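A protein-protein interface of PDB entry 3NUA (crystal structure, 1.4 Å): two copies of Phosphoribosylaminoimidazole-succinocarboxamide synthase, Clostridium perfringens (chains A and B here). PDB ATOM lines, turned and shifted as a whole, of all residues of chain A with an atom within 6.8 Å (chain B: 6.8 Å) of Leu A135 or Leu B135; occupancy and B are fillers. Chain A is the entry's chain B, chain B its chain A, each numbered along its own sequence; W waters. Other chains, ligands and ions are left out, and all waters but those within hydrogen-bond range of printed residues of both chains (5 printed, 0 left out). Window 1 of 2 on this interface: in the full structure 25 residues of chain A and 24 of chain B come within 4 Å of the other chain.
Water W4 lies within hydrogen-bond range of the backbone carbonyl oxygen of Ile A136 (2.7 Å), the side-chain amide nitrogen of Asn B137 (2.8 Å) and the backbone NH of Leu A124 (3.0 Å).
Water W1 lies within hydrogen-bond range of O of Ile B136 (2.7 Å), ND2 of Asn A137 (2.8 Å) and N of Leu B124 (2.9 Å).
Water W3 bridges the guanidinium group (NH2) of Arg A108 and a ring nitrogen (NE2) of His B140.
Water W5 bridges NH1 of Arg B108 (2.9 Å) and NE2 of His A140 (3.4 Å).
Water W2 lies within hydrogen-bond range of the side-chain carboxylate of Glu B123 (3.0 Å) and a ring nitrogen (NE2) of His A140 (3.4 Å).
Of the printed residues of chain B, Arg A108 touches Pro B134, Leu B135 and Ile B136.
Tyr A126 touches none of the printed residues of chain B.
Asp A133 touches none of the printed residues of chain B.
Of the printed residues of chain B, Leu A135 touches Arg B108 (2.7 Å) and Leu B135 (3.6 Å).
Of the printed residues of chain A, Ile B136 touches Arg A108 and Leu A109.
The nearest printed residue of chain B that does not touch Leu A135 is His B140 (4.01 Å).
The nearest printed residue of chain B that does not touch Glu A123 is Ile B136 (7.8 Å).
Arg A108 touches Leu B135, and with the chains exchanged Leu A135 touches Arg B108.
Arg A108 touches Ile B136, and with the chains exchanged Ile A136 touches Arg B108.
Leu A109 touches Pro B134, and with the chains exchanged Pro A134 touches Leu B109.
Glu A123 touches Asn B137, and with the chains exchanged Asn A137 touches Glu B123.
Positions printed for both chains: 98, 108, 109, 123, 124, 125, 126, 132, 133, 134, 135, 136, 137 and 140.
NE of Arg B98 lies within salt-bridge range of OE1 of Glu B123, 2.9 Å away.
O of Leu B124 is in hydrogen-bond range of N of Ile B136 (3.0 Å).
N of His B140 sits at hydrogen-bond distance from OD1 of Asn B137.
NE of Arg A98 is in salt-bridge range of OE1 of Glu A123, at 2.8 Å.
The backbone NH of Ile A136 lies within hydrogen-bond range of the backbone carbonyl oxygen of Leu A124 (3.0 Å).
N of Asn A137 lies within hydrogen-bond range of ND1 of His A140 (2.9 Å).
Of the 15 printed residues of chain A, 9 touch a printed residue of chain B.
Printed residues of chain A that touch a printed residue of chain B: Arg A108, Leu A109, Phe A122, Glu A123, Pro A134, Leu A135, Ile A136, Asn A137 and His A140.
Hydrophobic or aromatic side chains of chain A within 4 Å of the printed part of chain B: Leu A109, Pro A134, Leu A135, Ile A136 and His A140.
Hydrophobic or aromatic side chains of chain B that line the printed part of chain A: Leu B109, Pro B134, Leu B135, Ile B136 and His B140.
NH1 of Arg B108 lies within hydrogen-bond range of O of Leu A135, at 2.7 Å.
The side-chain carboxylate (OE1) of Glu B123 sits at hydrogen-bond distance from a ring nitrogen (NE2) of His A140 (2.8 Å).
The backbone carbonyl oxygen (O) of Leu B135 lies within hydrogen-bond range of the guanidinium group (NH2) of Arg A108 (2.8 Å).
The side-chain amide nitrogen (ND2) of Asn B137 sits at hydrogen-bond distance from the backbone carbonyl oxygen (O) of Phe A122.
NE2 of His B140 lies within hydrogen-bond range of OE1 of Glu A123, at 2.7 Å.
Among the printed residues, pairs that only touch across the chains: Glu A123 with Asn B137 (3.3 Å), Asn A137 with Glu B123 (3.3 Å), Leu A109 with Ile B136 (3.5 Å), Leu A135 with Leu B135 (3.6 Å), Ile A136 with Leu B109 (3.6 Å), Pro A134 with Arg B108 (3.7 Å), Pro A134 with Leu B109 (3.8 Å), Arg A108 with Pro B134 (3.8 Å), Leu A109 with Pro B134 (3.8 Å), Ile A136 with Arg B108 (3.9 Å) and Arg A108 with Ile B136 (3.97 Å).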
ATOM      1  N   ARG A  98     -12.714  -9.305  38.521  1.00  0.00           N
ATOM      2  CA  ARG A  98     -12.819  -7.841  38.530  1.00  0.00           C
ATOM      3  C   ARG A  98     -14.213  -7.454  38.992  1.00  0.00           C
ATOM      4  O   ARG A  98     -15.214  -7.761  38.338  1.00  0.00           O
ATOM      5  CB  ARG A  98     -12.529  -7.223  37.165  1.00  0.00           C
ATOM      6  CG  ARG A  98     -11.242  -7.656  36.534  1.00  0.00           C
ATOM      7  CD  ARG A  98     -11.011  -7.022  35.153  1.00  0.00           C
ATOM      8  NE  ARG A  98      -9.836  -7.641  34.543  1.00  0.00           N
ATOM      9  CZ  ARG A  98      -8.596  -7.217  34.744  1.00  0.00           C
ATOM     10  NH1 ARG A  98      -8.366  -6.116  35.475  1.00  0.00           N
ATOM     11  NH2 ARG A  98      -7.583  -7.853  34.190  1.00  0.00           N
ATOM     12  N   ARG A 108      -7.917  -1.414  27.666  1.00  0.00           N
ATOM     13  CA  ARG A 108      -8.126  -2.117  26.393  1.00  0.00           C
ATOM     14  C   ARG A 108      -9.574  -2.028  25.891  1.00  0.00           C
ATOM     15  O   ARG A 108      -9.835  -2.169  24.705  1.00  0.00           O
ATOM     16  CB  ARG A 108      -7.656  -3.571  26.444  1.00  0.00           C
ATOM     17  CG  ARG A 108      -8.478  -4.439  27.341  1.00  0.00           C
ATOM     18  CD  ARG A 108      -7.763  -5.777  27.738  1.00  0.00           C
ATOM     19  NE  ARG A 108      -7.423  -6.591  26.584  1.00  0.00           N
ATOM     20  CZ  ARG A 108      -8.316  -7.319  25.930  1.00  0.00           C
ATOM     21  NH1 ARG A 108      -7.949  -8.040  24.862  1.00  0.00           N
ATOM     22  NH2 ARG A 108      -9.571  -7.369  26.386  1.00  0.00           N
ATOM     23  N   LEU A 109     -10.516  -1.776  26.788  1.00  0.00           N
ATOM     24  CA  LEU A 109     -11.927  -1.690  26.420  1.00  0.00           C
ATOM     25  C   LEU A 109     -12.465  -0.262  26.364  1.00  0.00           C
ATOM     26  O   LEU A 109     -13.672  -0.058  26.191  1.00  0.00           O
ATOM     27  CB  LEU A 109     -12.788  -2.522  27.364  1.00  0.00           C
ATOM     28  CG  LEU A 109     -12.382  -3.989  27.376  1.00  0.00           C
ATOM     29  CD1 LEU A 109     -13.399  -4.778  28.148  1.00  0.00           C
ATOM     30  CD2 LEU A 109     -12.248  -4.548  25.953  1.00  0.00           C
ATOM     31  N   PHE A 122     -15.057 -12.577  35.598  1.00  0.00           N
ATOM     32  CA  PHE A 122     -14.100 -13.654  35.840  1.00  0.00           C
ATOM     33  C   PHE A 122     -13.347 -13.792  34.547  1.00  0.00           C
ATOM     34  O   PHE A 122     -13.956 -13.788  33.472  1.00  0.00           O
ATOM     35  CB  PHE A 122     -14.815 -14.982  36.194  1.00  0.00           C
ATOM     36  CG  PHE A 122     -15.627 -14.893  37.442  1.00  0.00           C
ATOM     37  CD1 PHE A 122     -15.090 -15.267  38.661  1.00  0.00           C
ATOM     38  CD2 PHE A 122     -16.922 -14.392  37.412  1.00  0.00           C
ATOM     39  CE1 PHE A 122     -15.840 -15.172  39.822  1.00  0.00           C
ATOM     40  CE2 PHE A 122     -17.662 -14.258  38.571  1.00  0.00           C
ATOM     41  CZ  PHE A 122     -17.126 -14.670  39.780  1.00  0.00           C
ATOM     42  N   GLU A 123     -12.034 -13.936  34.639  1.00  0.00           N
ATOM     43  CA  GLU A 123     -11.225 -14.103  33.465  1.00  0.00           C
ATOM     44  C   GLU A 123      -9.988 -14.956  33.725  1.00  0.00           C
ATOM     45  O   GLU A 123      -9.598 -15.168  34.882  1.00  0.00           O
ATOM     46  CB  GLU A 123     -10.919 -12.753  32.833  1.00  0.00           C
ATOM     47  CG  GLU A 123      -9.777 -12.073  33.457  1.00  0.00           C
ATOM     48  CD  GLU A 123      -9.520 -10.617  32.989  1.00  0.00           C
ATOM     49  OE1 GLU A 123     -10.445  -9.806  32.826  1.00  0.00           O
ATOM     50  OE2 GLU A 123      -8.341 -10.292  32.826  1.00  0.00           O
ATOM     51  N   LEU A 124      -9.377 -15.436  32.647  1.00  0.00           N
ATOM     52  CA  LEU A 124      -8.177 -16.235  32.702  1.00  0.00           C
ATOM     53  C   LEU A 124      -7.046 -15.565  31.967  1.00  0.00           C
ATOM     54  O   LEU A 124      -7.242 -14.999  30.898  1.00  0.00           O
ATOM     55  CB  LEU A 124      -8.402 -17.580  32.037  1.00  0.00           C
ATOM     56  CG  LEU A 124      -9.580 -18.416  32.521  1.00  0.00           C
ATOM     57  CD1 LEU A 124      -9.711 -19.693  31.719  1.00  0.00           C
ATOM     58  CD2 LEU A 124      -9.405 -18.777  34.004  1.00  0.00           C
ATOM     59  N   SER A 125      -5.856 -15.609  32.566  1.00  0.00           N
ATOM     60  CA  SER A 125      -4.642 -15.350  31.818  1.00  0.00           C
ATOM     61  C   SER A 125      -3.846 -16.646  31.773  1.00  0.00           C
ATOM     62  O   SER A 125      -3.821 -17.399  32.755  1.00  0.00           O
ATOM     63  CB  SER A 125      -3.837 -14.212  32.451  1.00  0.00           C
ATOM     64  OG  SER A 125      -4.236 -12.980  31.857  1.00  0.00           O
ATOM     65  N   TYR A 126      -3.228 -16.928  30.633  1.00  0.00           N
ATOM     66  CA  TYR A 126      -2.369 -18.095  30.513  1.00  0.00           C
ATOM     67  C   TYR A 126      -1.051 -17.785  31.203  1.00  0.00           C
ATOM     68  O   TYR A 126      -0.429 -16.769  30.910  1.00  0.00           O
ATOM     69  CB  TYR A 126      -2.146 -18.417  29.046  1.00  0.00           C
ATOM     70  CG  TYR A 126      -1.389 -19.684  28.776  1.00  0.00           C
ATOM     71  CD1 TYR A 126      -1.681 -20.847  29.468  1.00  0.00           C
ATOM     72  CD2 TYR A 126      -0.442 -19.743  27.764  1.00  0.00           C
ATOM     73  CE1 TYR A 126      -1.003 -22.020  29.211  1.00  0.00           C
ATOM     74  CE2 TYR A 126       0.228 -20.915  27.490  1.00  0.00           C
ATOM     75  CZ  TYR A 126      -0.052 -22.049  28.215  1.00  0.00           C
ATOM     76  OH  TYR A 126       0.613 -23.221  27.943  1.00  0.00           O
ATOM     77  N   GLY A 132       3.681 -12.991  27.689  1.00  0.00           N
ATOM     78  CA  GLY A 132       3.041 -11.864  28.337  1.00  0.00           C
ATOM     79  C   GLY A 132       1.766 -12.183  29.099  1.00  0.00           C
ATOM     80  O   GLY A 132       0.919 -11.297  29.282  1.00  0.00           O
ATOM     81  N   ASP A 133       1.607 -13.437  29.526  1.00  0.00           N
ATOM     82  CA  ASP A 133       0.428 -13.855  30.300  1.00  0.00           C
ATOM     83  C   ASP A 133      -0.852 -13.416  29.611  1.00  0.00           C
ATOM     84  O   ASP A 133      -1.654 -12.666  30.185  1.00  0.00           O
ATOM     85  CB  ASP A 133       0.475 -13.268  31.721  1.00  0.00           C
ATOM     86  CG  ASP A 133       1.758 -13.630  32.461  1.00  0.00           C
ATOM     87  OD1 ASP A 133       2.168 -14.799  32.382  1.00  0.00           O
ATOM     88  OD2 ASP A 133       2.372 -12.739  33.112  1.00  0.00           O
ATOM     89  N   PRO A 134      -1.075 -13.905  28.382  1.00  0.00           N
ATOM     90  CA  PRO A 134      -2.211 -13.414  27.602  1.00  0.00           C
ATOM     91  C   PRO A 134      -3.564 -13.808  28.168  1.00  0.00           C
ATOM     92  O   PRO A 134      -3.750 -14.940  28.639  1.00  0.00           O
ATOM     93  CB  PRO A 134      -2.011 -14.073  26.230  1.00  0.00           C
ATOM     94  CG  PRO A 134      -1.239 -15.313  26.513  1.00  0.00           C
ATOM     95  CD  PRO A 134      -0.288 -14.902  27.634  1.00  0.00           C
ATOM     96  N   LEU A 135      -4.509 -12.878  28.088  1.00  0.00           N
ATOM     97  CA  LEU A 135      -5.915 -13.171  28.278  1.00  0.00           C
ATOM     98  C   LEU A 135      -6.315 -14.320  27.364  1.00  0.00           C
ATOM     99  O   LEU A 135      -6.061 -14.271  26.148  1.00  0.00           O
ATOM    100  CB  LEU A 135      -6.764 -11.925  27.961  1.00  0.00           C
ATOM    101  CG  LEU A 135      -8.281 -12.136  27.938  1.00  0.00           C
ATOM    102  CD1 LEU A 135      -8.867 -12.387  29.319  1.00  0.00           C
ATOM    103  CD2 LEU A 135      -8.980 -10.945  27.324  1.00  0.00           C
ATOM    104  N   ILE A 136      -6.956 -15.337  27.937  1.00  0.00           N
ATOM    105  CA  ILE A 136      -7.567 -16.395  27.133  1.00  0.00           C
ATOM    106  C   ILE A 136      -8.937 -16.734  27.696  1.00  0.00           C
ATOM    107  O   ILE A 136      -9.229 -16.403  28.851  1.00  0.00           O
ATOM    108  CB  ILE A 136      -6.711 -17.672  27.133  1.00  0.00           C
ATOM    109  CG1 ILE A 136      -6.521 -18.234  28.552  1.00  0.00           C
ATOM    110  CG2 ILE A 136      -5.362 -17.416  26.445  1.00  0.00           C
ATOM    111  CD1 ILE A 136      -5.863 -19.643  28.506  1.00  0.00           C
ATOM    112  N   ASN A 137      -9.765 -17.394  26.882  1.00  0.00           N
ATOM    113  CA  ASN A 137     -11.065 -17.840  27.359  1.00  0.00           C
ATOM    114  C   ASN A 137     -11.069 -19.337  27.686  1.00  0.00           C
ATOM    115  O   ASN A 137     -10.033 -20.008  27.545  1.00  0.00           O
ATOM    116  CB  ASN A 137     -12.219 -17.414  26.435  1.00  0.00           C
ATOM    117  CG  ASN A 137     -12.301 -18.207  25.144  1.00  0.00           C
ATOM    118  OD1 ASN A 137     -11.950 -19.381  25.082  1.00  0.00           O
ATOM    119  ND2 ASN A 137     -12.851 -17.580  24.105  1.00  0.00           N
ATOM    120  N   HIS A 140     -10.122 -21.652  24.810  1.00  0.00           N
ATOM    121  CA  HIS A 140      -8.686 -21.669  24.543  1.00  0.00           C
ATOM    122  C   HIS A 140      -7.985 -22.555  25.573  1.00  0.00           C
ATOM    123  O   HIS A 140      -7.085 -23.335  25.232  1.00  0.00           O
ATOM    124  CB  HIS A 140      -8.094 -20.271  24.664  1.00  0.00           C
ATOM    125  CG  HIS A 140      -8.686 -19.262  23.731  1.00  0.00           C
ATOM    126  ND1 HIS A 140      -9.006 -17.987  24.138  1.00  0.00           N
ATOM    127  CD2 HIS A 140      -8.984 -19.320  22.409  1.00  0.00           C
ATOM    128  CE1 HIS A 140      -9.481 -17.304  23.112  1.00  0.00           C
ATOM    129  NE2 HIS A 140      -9.477 -18.086  22.046  1.00  0.00           N
ATOM    130  N   ARG B  98     -12.954 -21.273  16.002  1.00  0.00           N
ATOM    131  CA  ARG B  98     -11.696 -21.846  15.509  1.00  0.00           C
ATOM    132  C   ARG B  98     -11.769 -23.347  15.655  1.00  0.00           C
ATOM    133  O   ARG B  98     -11.840 -23.866  16.766  1.00  0.00           O
ATOM    134  CB  ARG B  98     -10.457 -21.286  16.229  1.00  0.00           C
ATOM    135  CG  ARG B  98     -10.422 -19.771  16.344  1.00  0.00           C
ATOM    136  CD  ARG B  98      -9.146 -19.306  17.103  1.00  0.00           C
ATOM    137  NE  ARG B  98      -9.200 -17.855  17.244  1.00  0.00           N
ATOM    138  CZ  ARG B  98      -8.752 -16.981  16.350  1.00  0.00           C
ATOM    139  NH1 ARG B  98      -8.101 -17.390  15.256  1.00  0.00           N
ATOM    140  NH2 ARG B  98      -8.946 -15.681  16.567  1.00  0.00           N
ATOM    141  N   ARG B 108      -0.512 -15.628  19.394  1.00  0.00           N
ATOM    142  CA  ARG B 108      -0.463 -15.132  20.764  1.00  0.00           C
ATOM    143  C   ARG B 108      -0.241 -16.241  21.794  1.00  0.00           C
ATOM    144  O   ARG B 108       0.210 -15.968  22.914  1.00  0.00           O
ATOM    145  CB  ARG B 108      -1.716 -14.309  21.088  1.00  0.00           C
ATOM    146  CG  ARG B 108      -2.950 -15.137  21.213  1.00  0.00           C
ATOM    147  CD  ARG B 108      -4.236 -14.255  21.060  1.00  0.00           C
ATOM    148  NE  ARG B 108      -4.329 -13.259  22.116  1.00  0.00           N
ATOM    149  CZ  ARG B 108      -4.785 -13.529  23.331  1.00  0.00           C
ATOM    150  NH1 ARG B 108      -5.209 -14.759  23.585  1.00  0.00           N
ATOM    151  NH2 ARG B 108      -4.816 -12.580  24.289  1.00  0.00           N
ATOM    152  N   LEU B 109      -0.550 -17.489  21.430  1.00  0.00           N
ATOM    153  CA  LEU B 109      -0.312 -18.598  22.351  1.00  0.00           C
ATOM    154  C   LEU B 109       0.926 -19.410  21.973  1.00  0.00           C
ATOM    155  O   LEU B 109       1.224 -20.448  22.584  1.00  0.00           O
ATOM    156  CB  LEU B 109      -1.542 -19.485  22.443  1.00  0.00           C
ATOM    157  CG  LEU B 109      -2.784 -18.752  22.966  1.00  0.00           C
ATOM    158  CD1 LEU B 109      -3.987 -19.694  23.079  1.00  0.00           C
ATOM    159  CD2 LEU B 109      -2.544 -18.064  24.305  1.00  0.00           C
ATOM    160  N   GLU B 123     -15.072 -17.717  20.487  1.00  0.00           N
ATOM    161  CA  GLU B 123     -14.521 -16.548  21.147  1.00  0.00           C
ATOM    162  C   GLU B 123     -15.192 -15.290  20.669  1.00  0.00           C
ATOM    163  O   GLU B 123     -15.842 -15.273  19.611  1.00  0.00           O
ATOM    164  CB  GLU B 123     -13.013 -16.525  20.963  1.00  0.00           C
ATOM    165  CG  GLU B 123     -12.578 -16.024  19.646  1.00  0.00           C
ATOM    166  CD  GLU B 123     -11.091 -15.992  19.404  1.00  0.00           C
ATOM    167  OE1 GLU B 123     -10.382 -16.968  19.690  1.00  0.00           O
ATOM    168  OE2 GLU B 123     -10.630 -15.019  18.779  1.00  0.00           O
ATOM    169  N   LEU B 124     -15.023 -14.220  21.435  1.00  0.00           N
ATOM    170  CA  LEU B 124     -15.563 -12.931  21.076  1.00  0.00           C
ATOM    171  C   LEU B 124     -14.487 -11.898  20.875  1.00  0.00           C
ATOM    172  O   LEU B 124     -13.513 -11.842  21.625  1.00  0.00           O
ATOM    173  CB  LEU B 124     -16.421 -12.401  22.221  1.00  0.00           C
ATOM    174  CG  LEU B 124     -17.577 -13.294  22.643  1.00  0.00           C
ATOM    175  CD1 LEU B 124     -18.283 -12.644  23.836  1.00  0.00           C
ATOM    176  CD2 LEU B 124     -18.575 -13.564  21.474  1.00  0.00           C
ATOM    177  N   SER B 125     -14.667 -11.061  19.862  1.00  0.00           N
ATOM    178  CA  SER B 125     -13.952  -9.790  19.830  1.00  0.00           C
ATOM    179  C   SER B 125     -14.977  -8.673  19.944  1.00  0.00           C
ATOM    180  O   SER B 125     -16.081  -8.743  19.398  1.00  0.00           O
ATOM    181  CB  SER B 125     -13.122  -9.659  18.549  1.00  0.00           C
ATOM    182  OG  SER B 125     -11.832 -10.240  18.767  1.00  0.00           O
ATOM    183  N   TYR B 126     -14.609  -7.625  20.662  1.00  0.00           N
ATOM    184  CA  TYR B 126     -15.490  -6.469  20.768  1.00  0.00           C
ATOM    185  C   TYR B 126     -15.416  -5.681  19.461  1.00  0.00           C
ATOM    186  O   TYR B 126     -14.316  -5.374  19.009  1.00  0.00           O
ATOM    187  CB  TYR B 126     -15.000  -5.624  21.948  1.00  0.00           C
ATOM    188  CG  TYR B 126     -15.894  -4.460  22.299  1.00  0.00           C
ATOM    189  CD1 TYR B 126     -17.273  -4.565  22.238  1.00  0.00           C
ATOM    190  CD2 TYR B 126     -15.332  -3.278  22.747  1.00  0.00           C
ATOM    191  CE1 TYR B 126     -18.092  -3.511  22.559  1.00  0.00           C
ATOM    192  CE2 TYR B 126     -16.125  -2.217  23.093  1.00  0.00           C
ATOM    193  CZ  TYR B 126     -17.506  -2.334  22.988  1.00  0.00           C
ATOM    194  OH  TYR B 126     -18.265  -1.252  23.353  1.00  0.00           O
ATOM    195  N   GLY B 132      -9.127  -1.673  18.184  1.00  0.00           N
ATOM    196  CA  GLY B 132      -8.470  -2.808  17.569  1.00  0.00           C
ATOM    197  C   GLY B 132      -9.241  -4.119  17.703  1.00  0.00           C
ATOM    198  O   GLY B 132      -8.638  -5.182  17.587  1.00  0.00           O
ATOM    199  N   ASP B 133     -10.558  -4.053  17.919  1.00  0.00           N
ATOM    200  CA  ASP B 133     -11.399  -5.262  18.014  1.00  0.00           C
ATOM    201  C   ASP B 133     -10.788  -6.255  19.004  1.00  0.00           C
ATOM    202  O   ASP B 133     -10.470  -7.399  18.653  1.00  0.00           O
ATOM    203  CB  ASP B 133     -11.564  -5.927  16.642  1.00  0.00           C
ATOM    204  CG  ASP B 133     -12.215  -5.023  15.616  1.00  0.00           C
ATOM    205  OD1 ASP B 133     -13.056  -4.173  15.966  1.00  0.00           O
ATOM    206  OD2 ASP B 133     -11.893  -5.193  14.429  1.00  0.00           O
ATOM    207  N   PRO B 134     -10.643  -5.836  20.261  1.00  0.00           N
ATOM    208  CA  PRO B 134      -9.946  -6.689  21.231  1.00  0.00           C
ATOM    209  C   PRO B 134     -10.695  -7.970  21.577  1.00  0.00           C
ATOM    210  O   PRO B 134     -11.924  -7.965  21.672  1.00  0.00           O
ATOM    211  CB  PRO B 134      -9.867  -5.793  22.475  1.00  0.00           C
ATOM    212  CG  PRO B 134     -11.047  -4.879  22.347  1.00  0.00           C
ATOM    213  CD  PRO B 134     -11.153  -4.598  20.874  1.00  0.00           C
ATOM    214  N   LEU B 135      -9.942  -9.039  21.803  1.00  0.00           N
ATOM    215  CA  LEU B 135     -10.477 -10.258  22.408  1.00  0.00           C
ATOM    216  C   LEU B 135     -11.105  -9.938  23.750  1.00  0.00           C
ATOM    217  O   LEU B 135     -10.483  -9.275  24.568  1.00  0.00           O
ATOM    218  CB  LEU B 135      -9.372 -11.290  22.581  1.00  0.00           C
ATOM    219  CG  LEU B 135      -9.731 -12.562  23.358  1.00  0.00           C
ATOM    220  CD1 LEU B 135     -10.657 -13.423  22.588  1.00  0.00           C
ATOM    221  CD2 LEU B 135      -8.476 -13.365  23.669  1.00  0.00           C
ATOM    222  N   ILE B 136     -12.332 -10.418  23.978  1.00  0.00           N
ATOM    223  CA  ILE B 136     -12.989 -10.287  25.280  1.00  0.00           C
ATOM    224  C   ILE B 136     -13.666 -11.590  25.625  1.00  0.00           C
ATOM    225  O   ILE B 136     -13.909 -12.389  24.729  1.00  0.00           O
ATOM    226  CB  ILE B 136     -14.019  -9.134  25.336  1.00  0.00           C
ATOM    227  CG1 ILE B 136     -15.118  -9.306  24.292  1.00  0.00           C
ATOM    228  CG2 ILE B 136     -13.319  -7.790  25.139  1.00  0.00           C
ATOM    229  CD1 ILE B 136     -16.255  -8.342  24.533  1.00  0.00           C
ATOM    230  N   ASN B 137     -14.010 -11.791  26.883  1.00  0.00           N
ATOM    231  CA  ASN B 137     -14.770 -12.974  27.241  1.00  0.00           C
ATOM    232  C   ASN B 137     -16.235 -12.617  27.527  1.00  0.00           C
ATOM    233  O   ASN B 137     -16.631 -11.450  27.372  1.00  0.00           O
ATOM    234  CB  ASN B 137     -14.060 -13.755  28.373  1.00  0.00           C
ATOM    235  CG  ASN B 137     -14.184 -13.103  29.743  1.00  0.00           C
ATOM    236  OD1 ASN B 137     -15.145 -12.354  30.032  1.00  0.00           O
ATOM    237  ND2 ASN B 137     -13.228 -13.414  30.617  1.00  0.00           N
ATOM    238  N   HIS B 140     -16.806  -9.946  30.238  1.00  0.00           N
ATOM    239  CA  HIS B 140     -16.524  -8.601  29.750  1.00  0.00           C
ATOM    240  C   HIS B 140     -17.693  -8.098  28.912  1.00  0.00           C
ATOM    241  O   HIS B 140     -18.101  -6.937  29.069  1.00  0.00           O
ATOM    242  CB  HIS B 140     -15.290  -8.579  28.866  1.00  0.00           C
ATOM    243  CG  HIS B 140     -14.049  -9.040  29.550  1.00  0.00           C
ATOM    244  ND1 HIS B 140     -13.129  -9.860  28.935  1.00  0.00           N
ATOM    245  CD2 HIS B 140     -13.573  -8.792  30.791  1.00  0.00           C
ATOM    246  CE1 HIS B 140     -12.139 -10.110  29.776  1.00  0.00           C
ATOM    247  NE2 HIS B 140     -12.379  -9.468  30.909  1.00  0.00           N
HETATM  248  O   HOH W   1     -14.009 -14.979  24.093  1.00  0.00           O
HETATM  249  O   HOH W   2      -7.627 -15.947  20.077  1.00  0.00           O
HETATM  250  O   HOH W   3     -10.997  -7.199  28.895  1.00  0.00           O
HETATM  251  O   HOH W   4     -11.212 -15.364  30.288  1.00  0.00           O
HETATM  252  O   HOH W   5      -6.247 -17.038  22.098  1.00  0.00           O
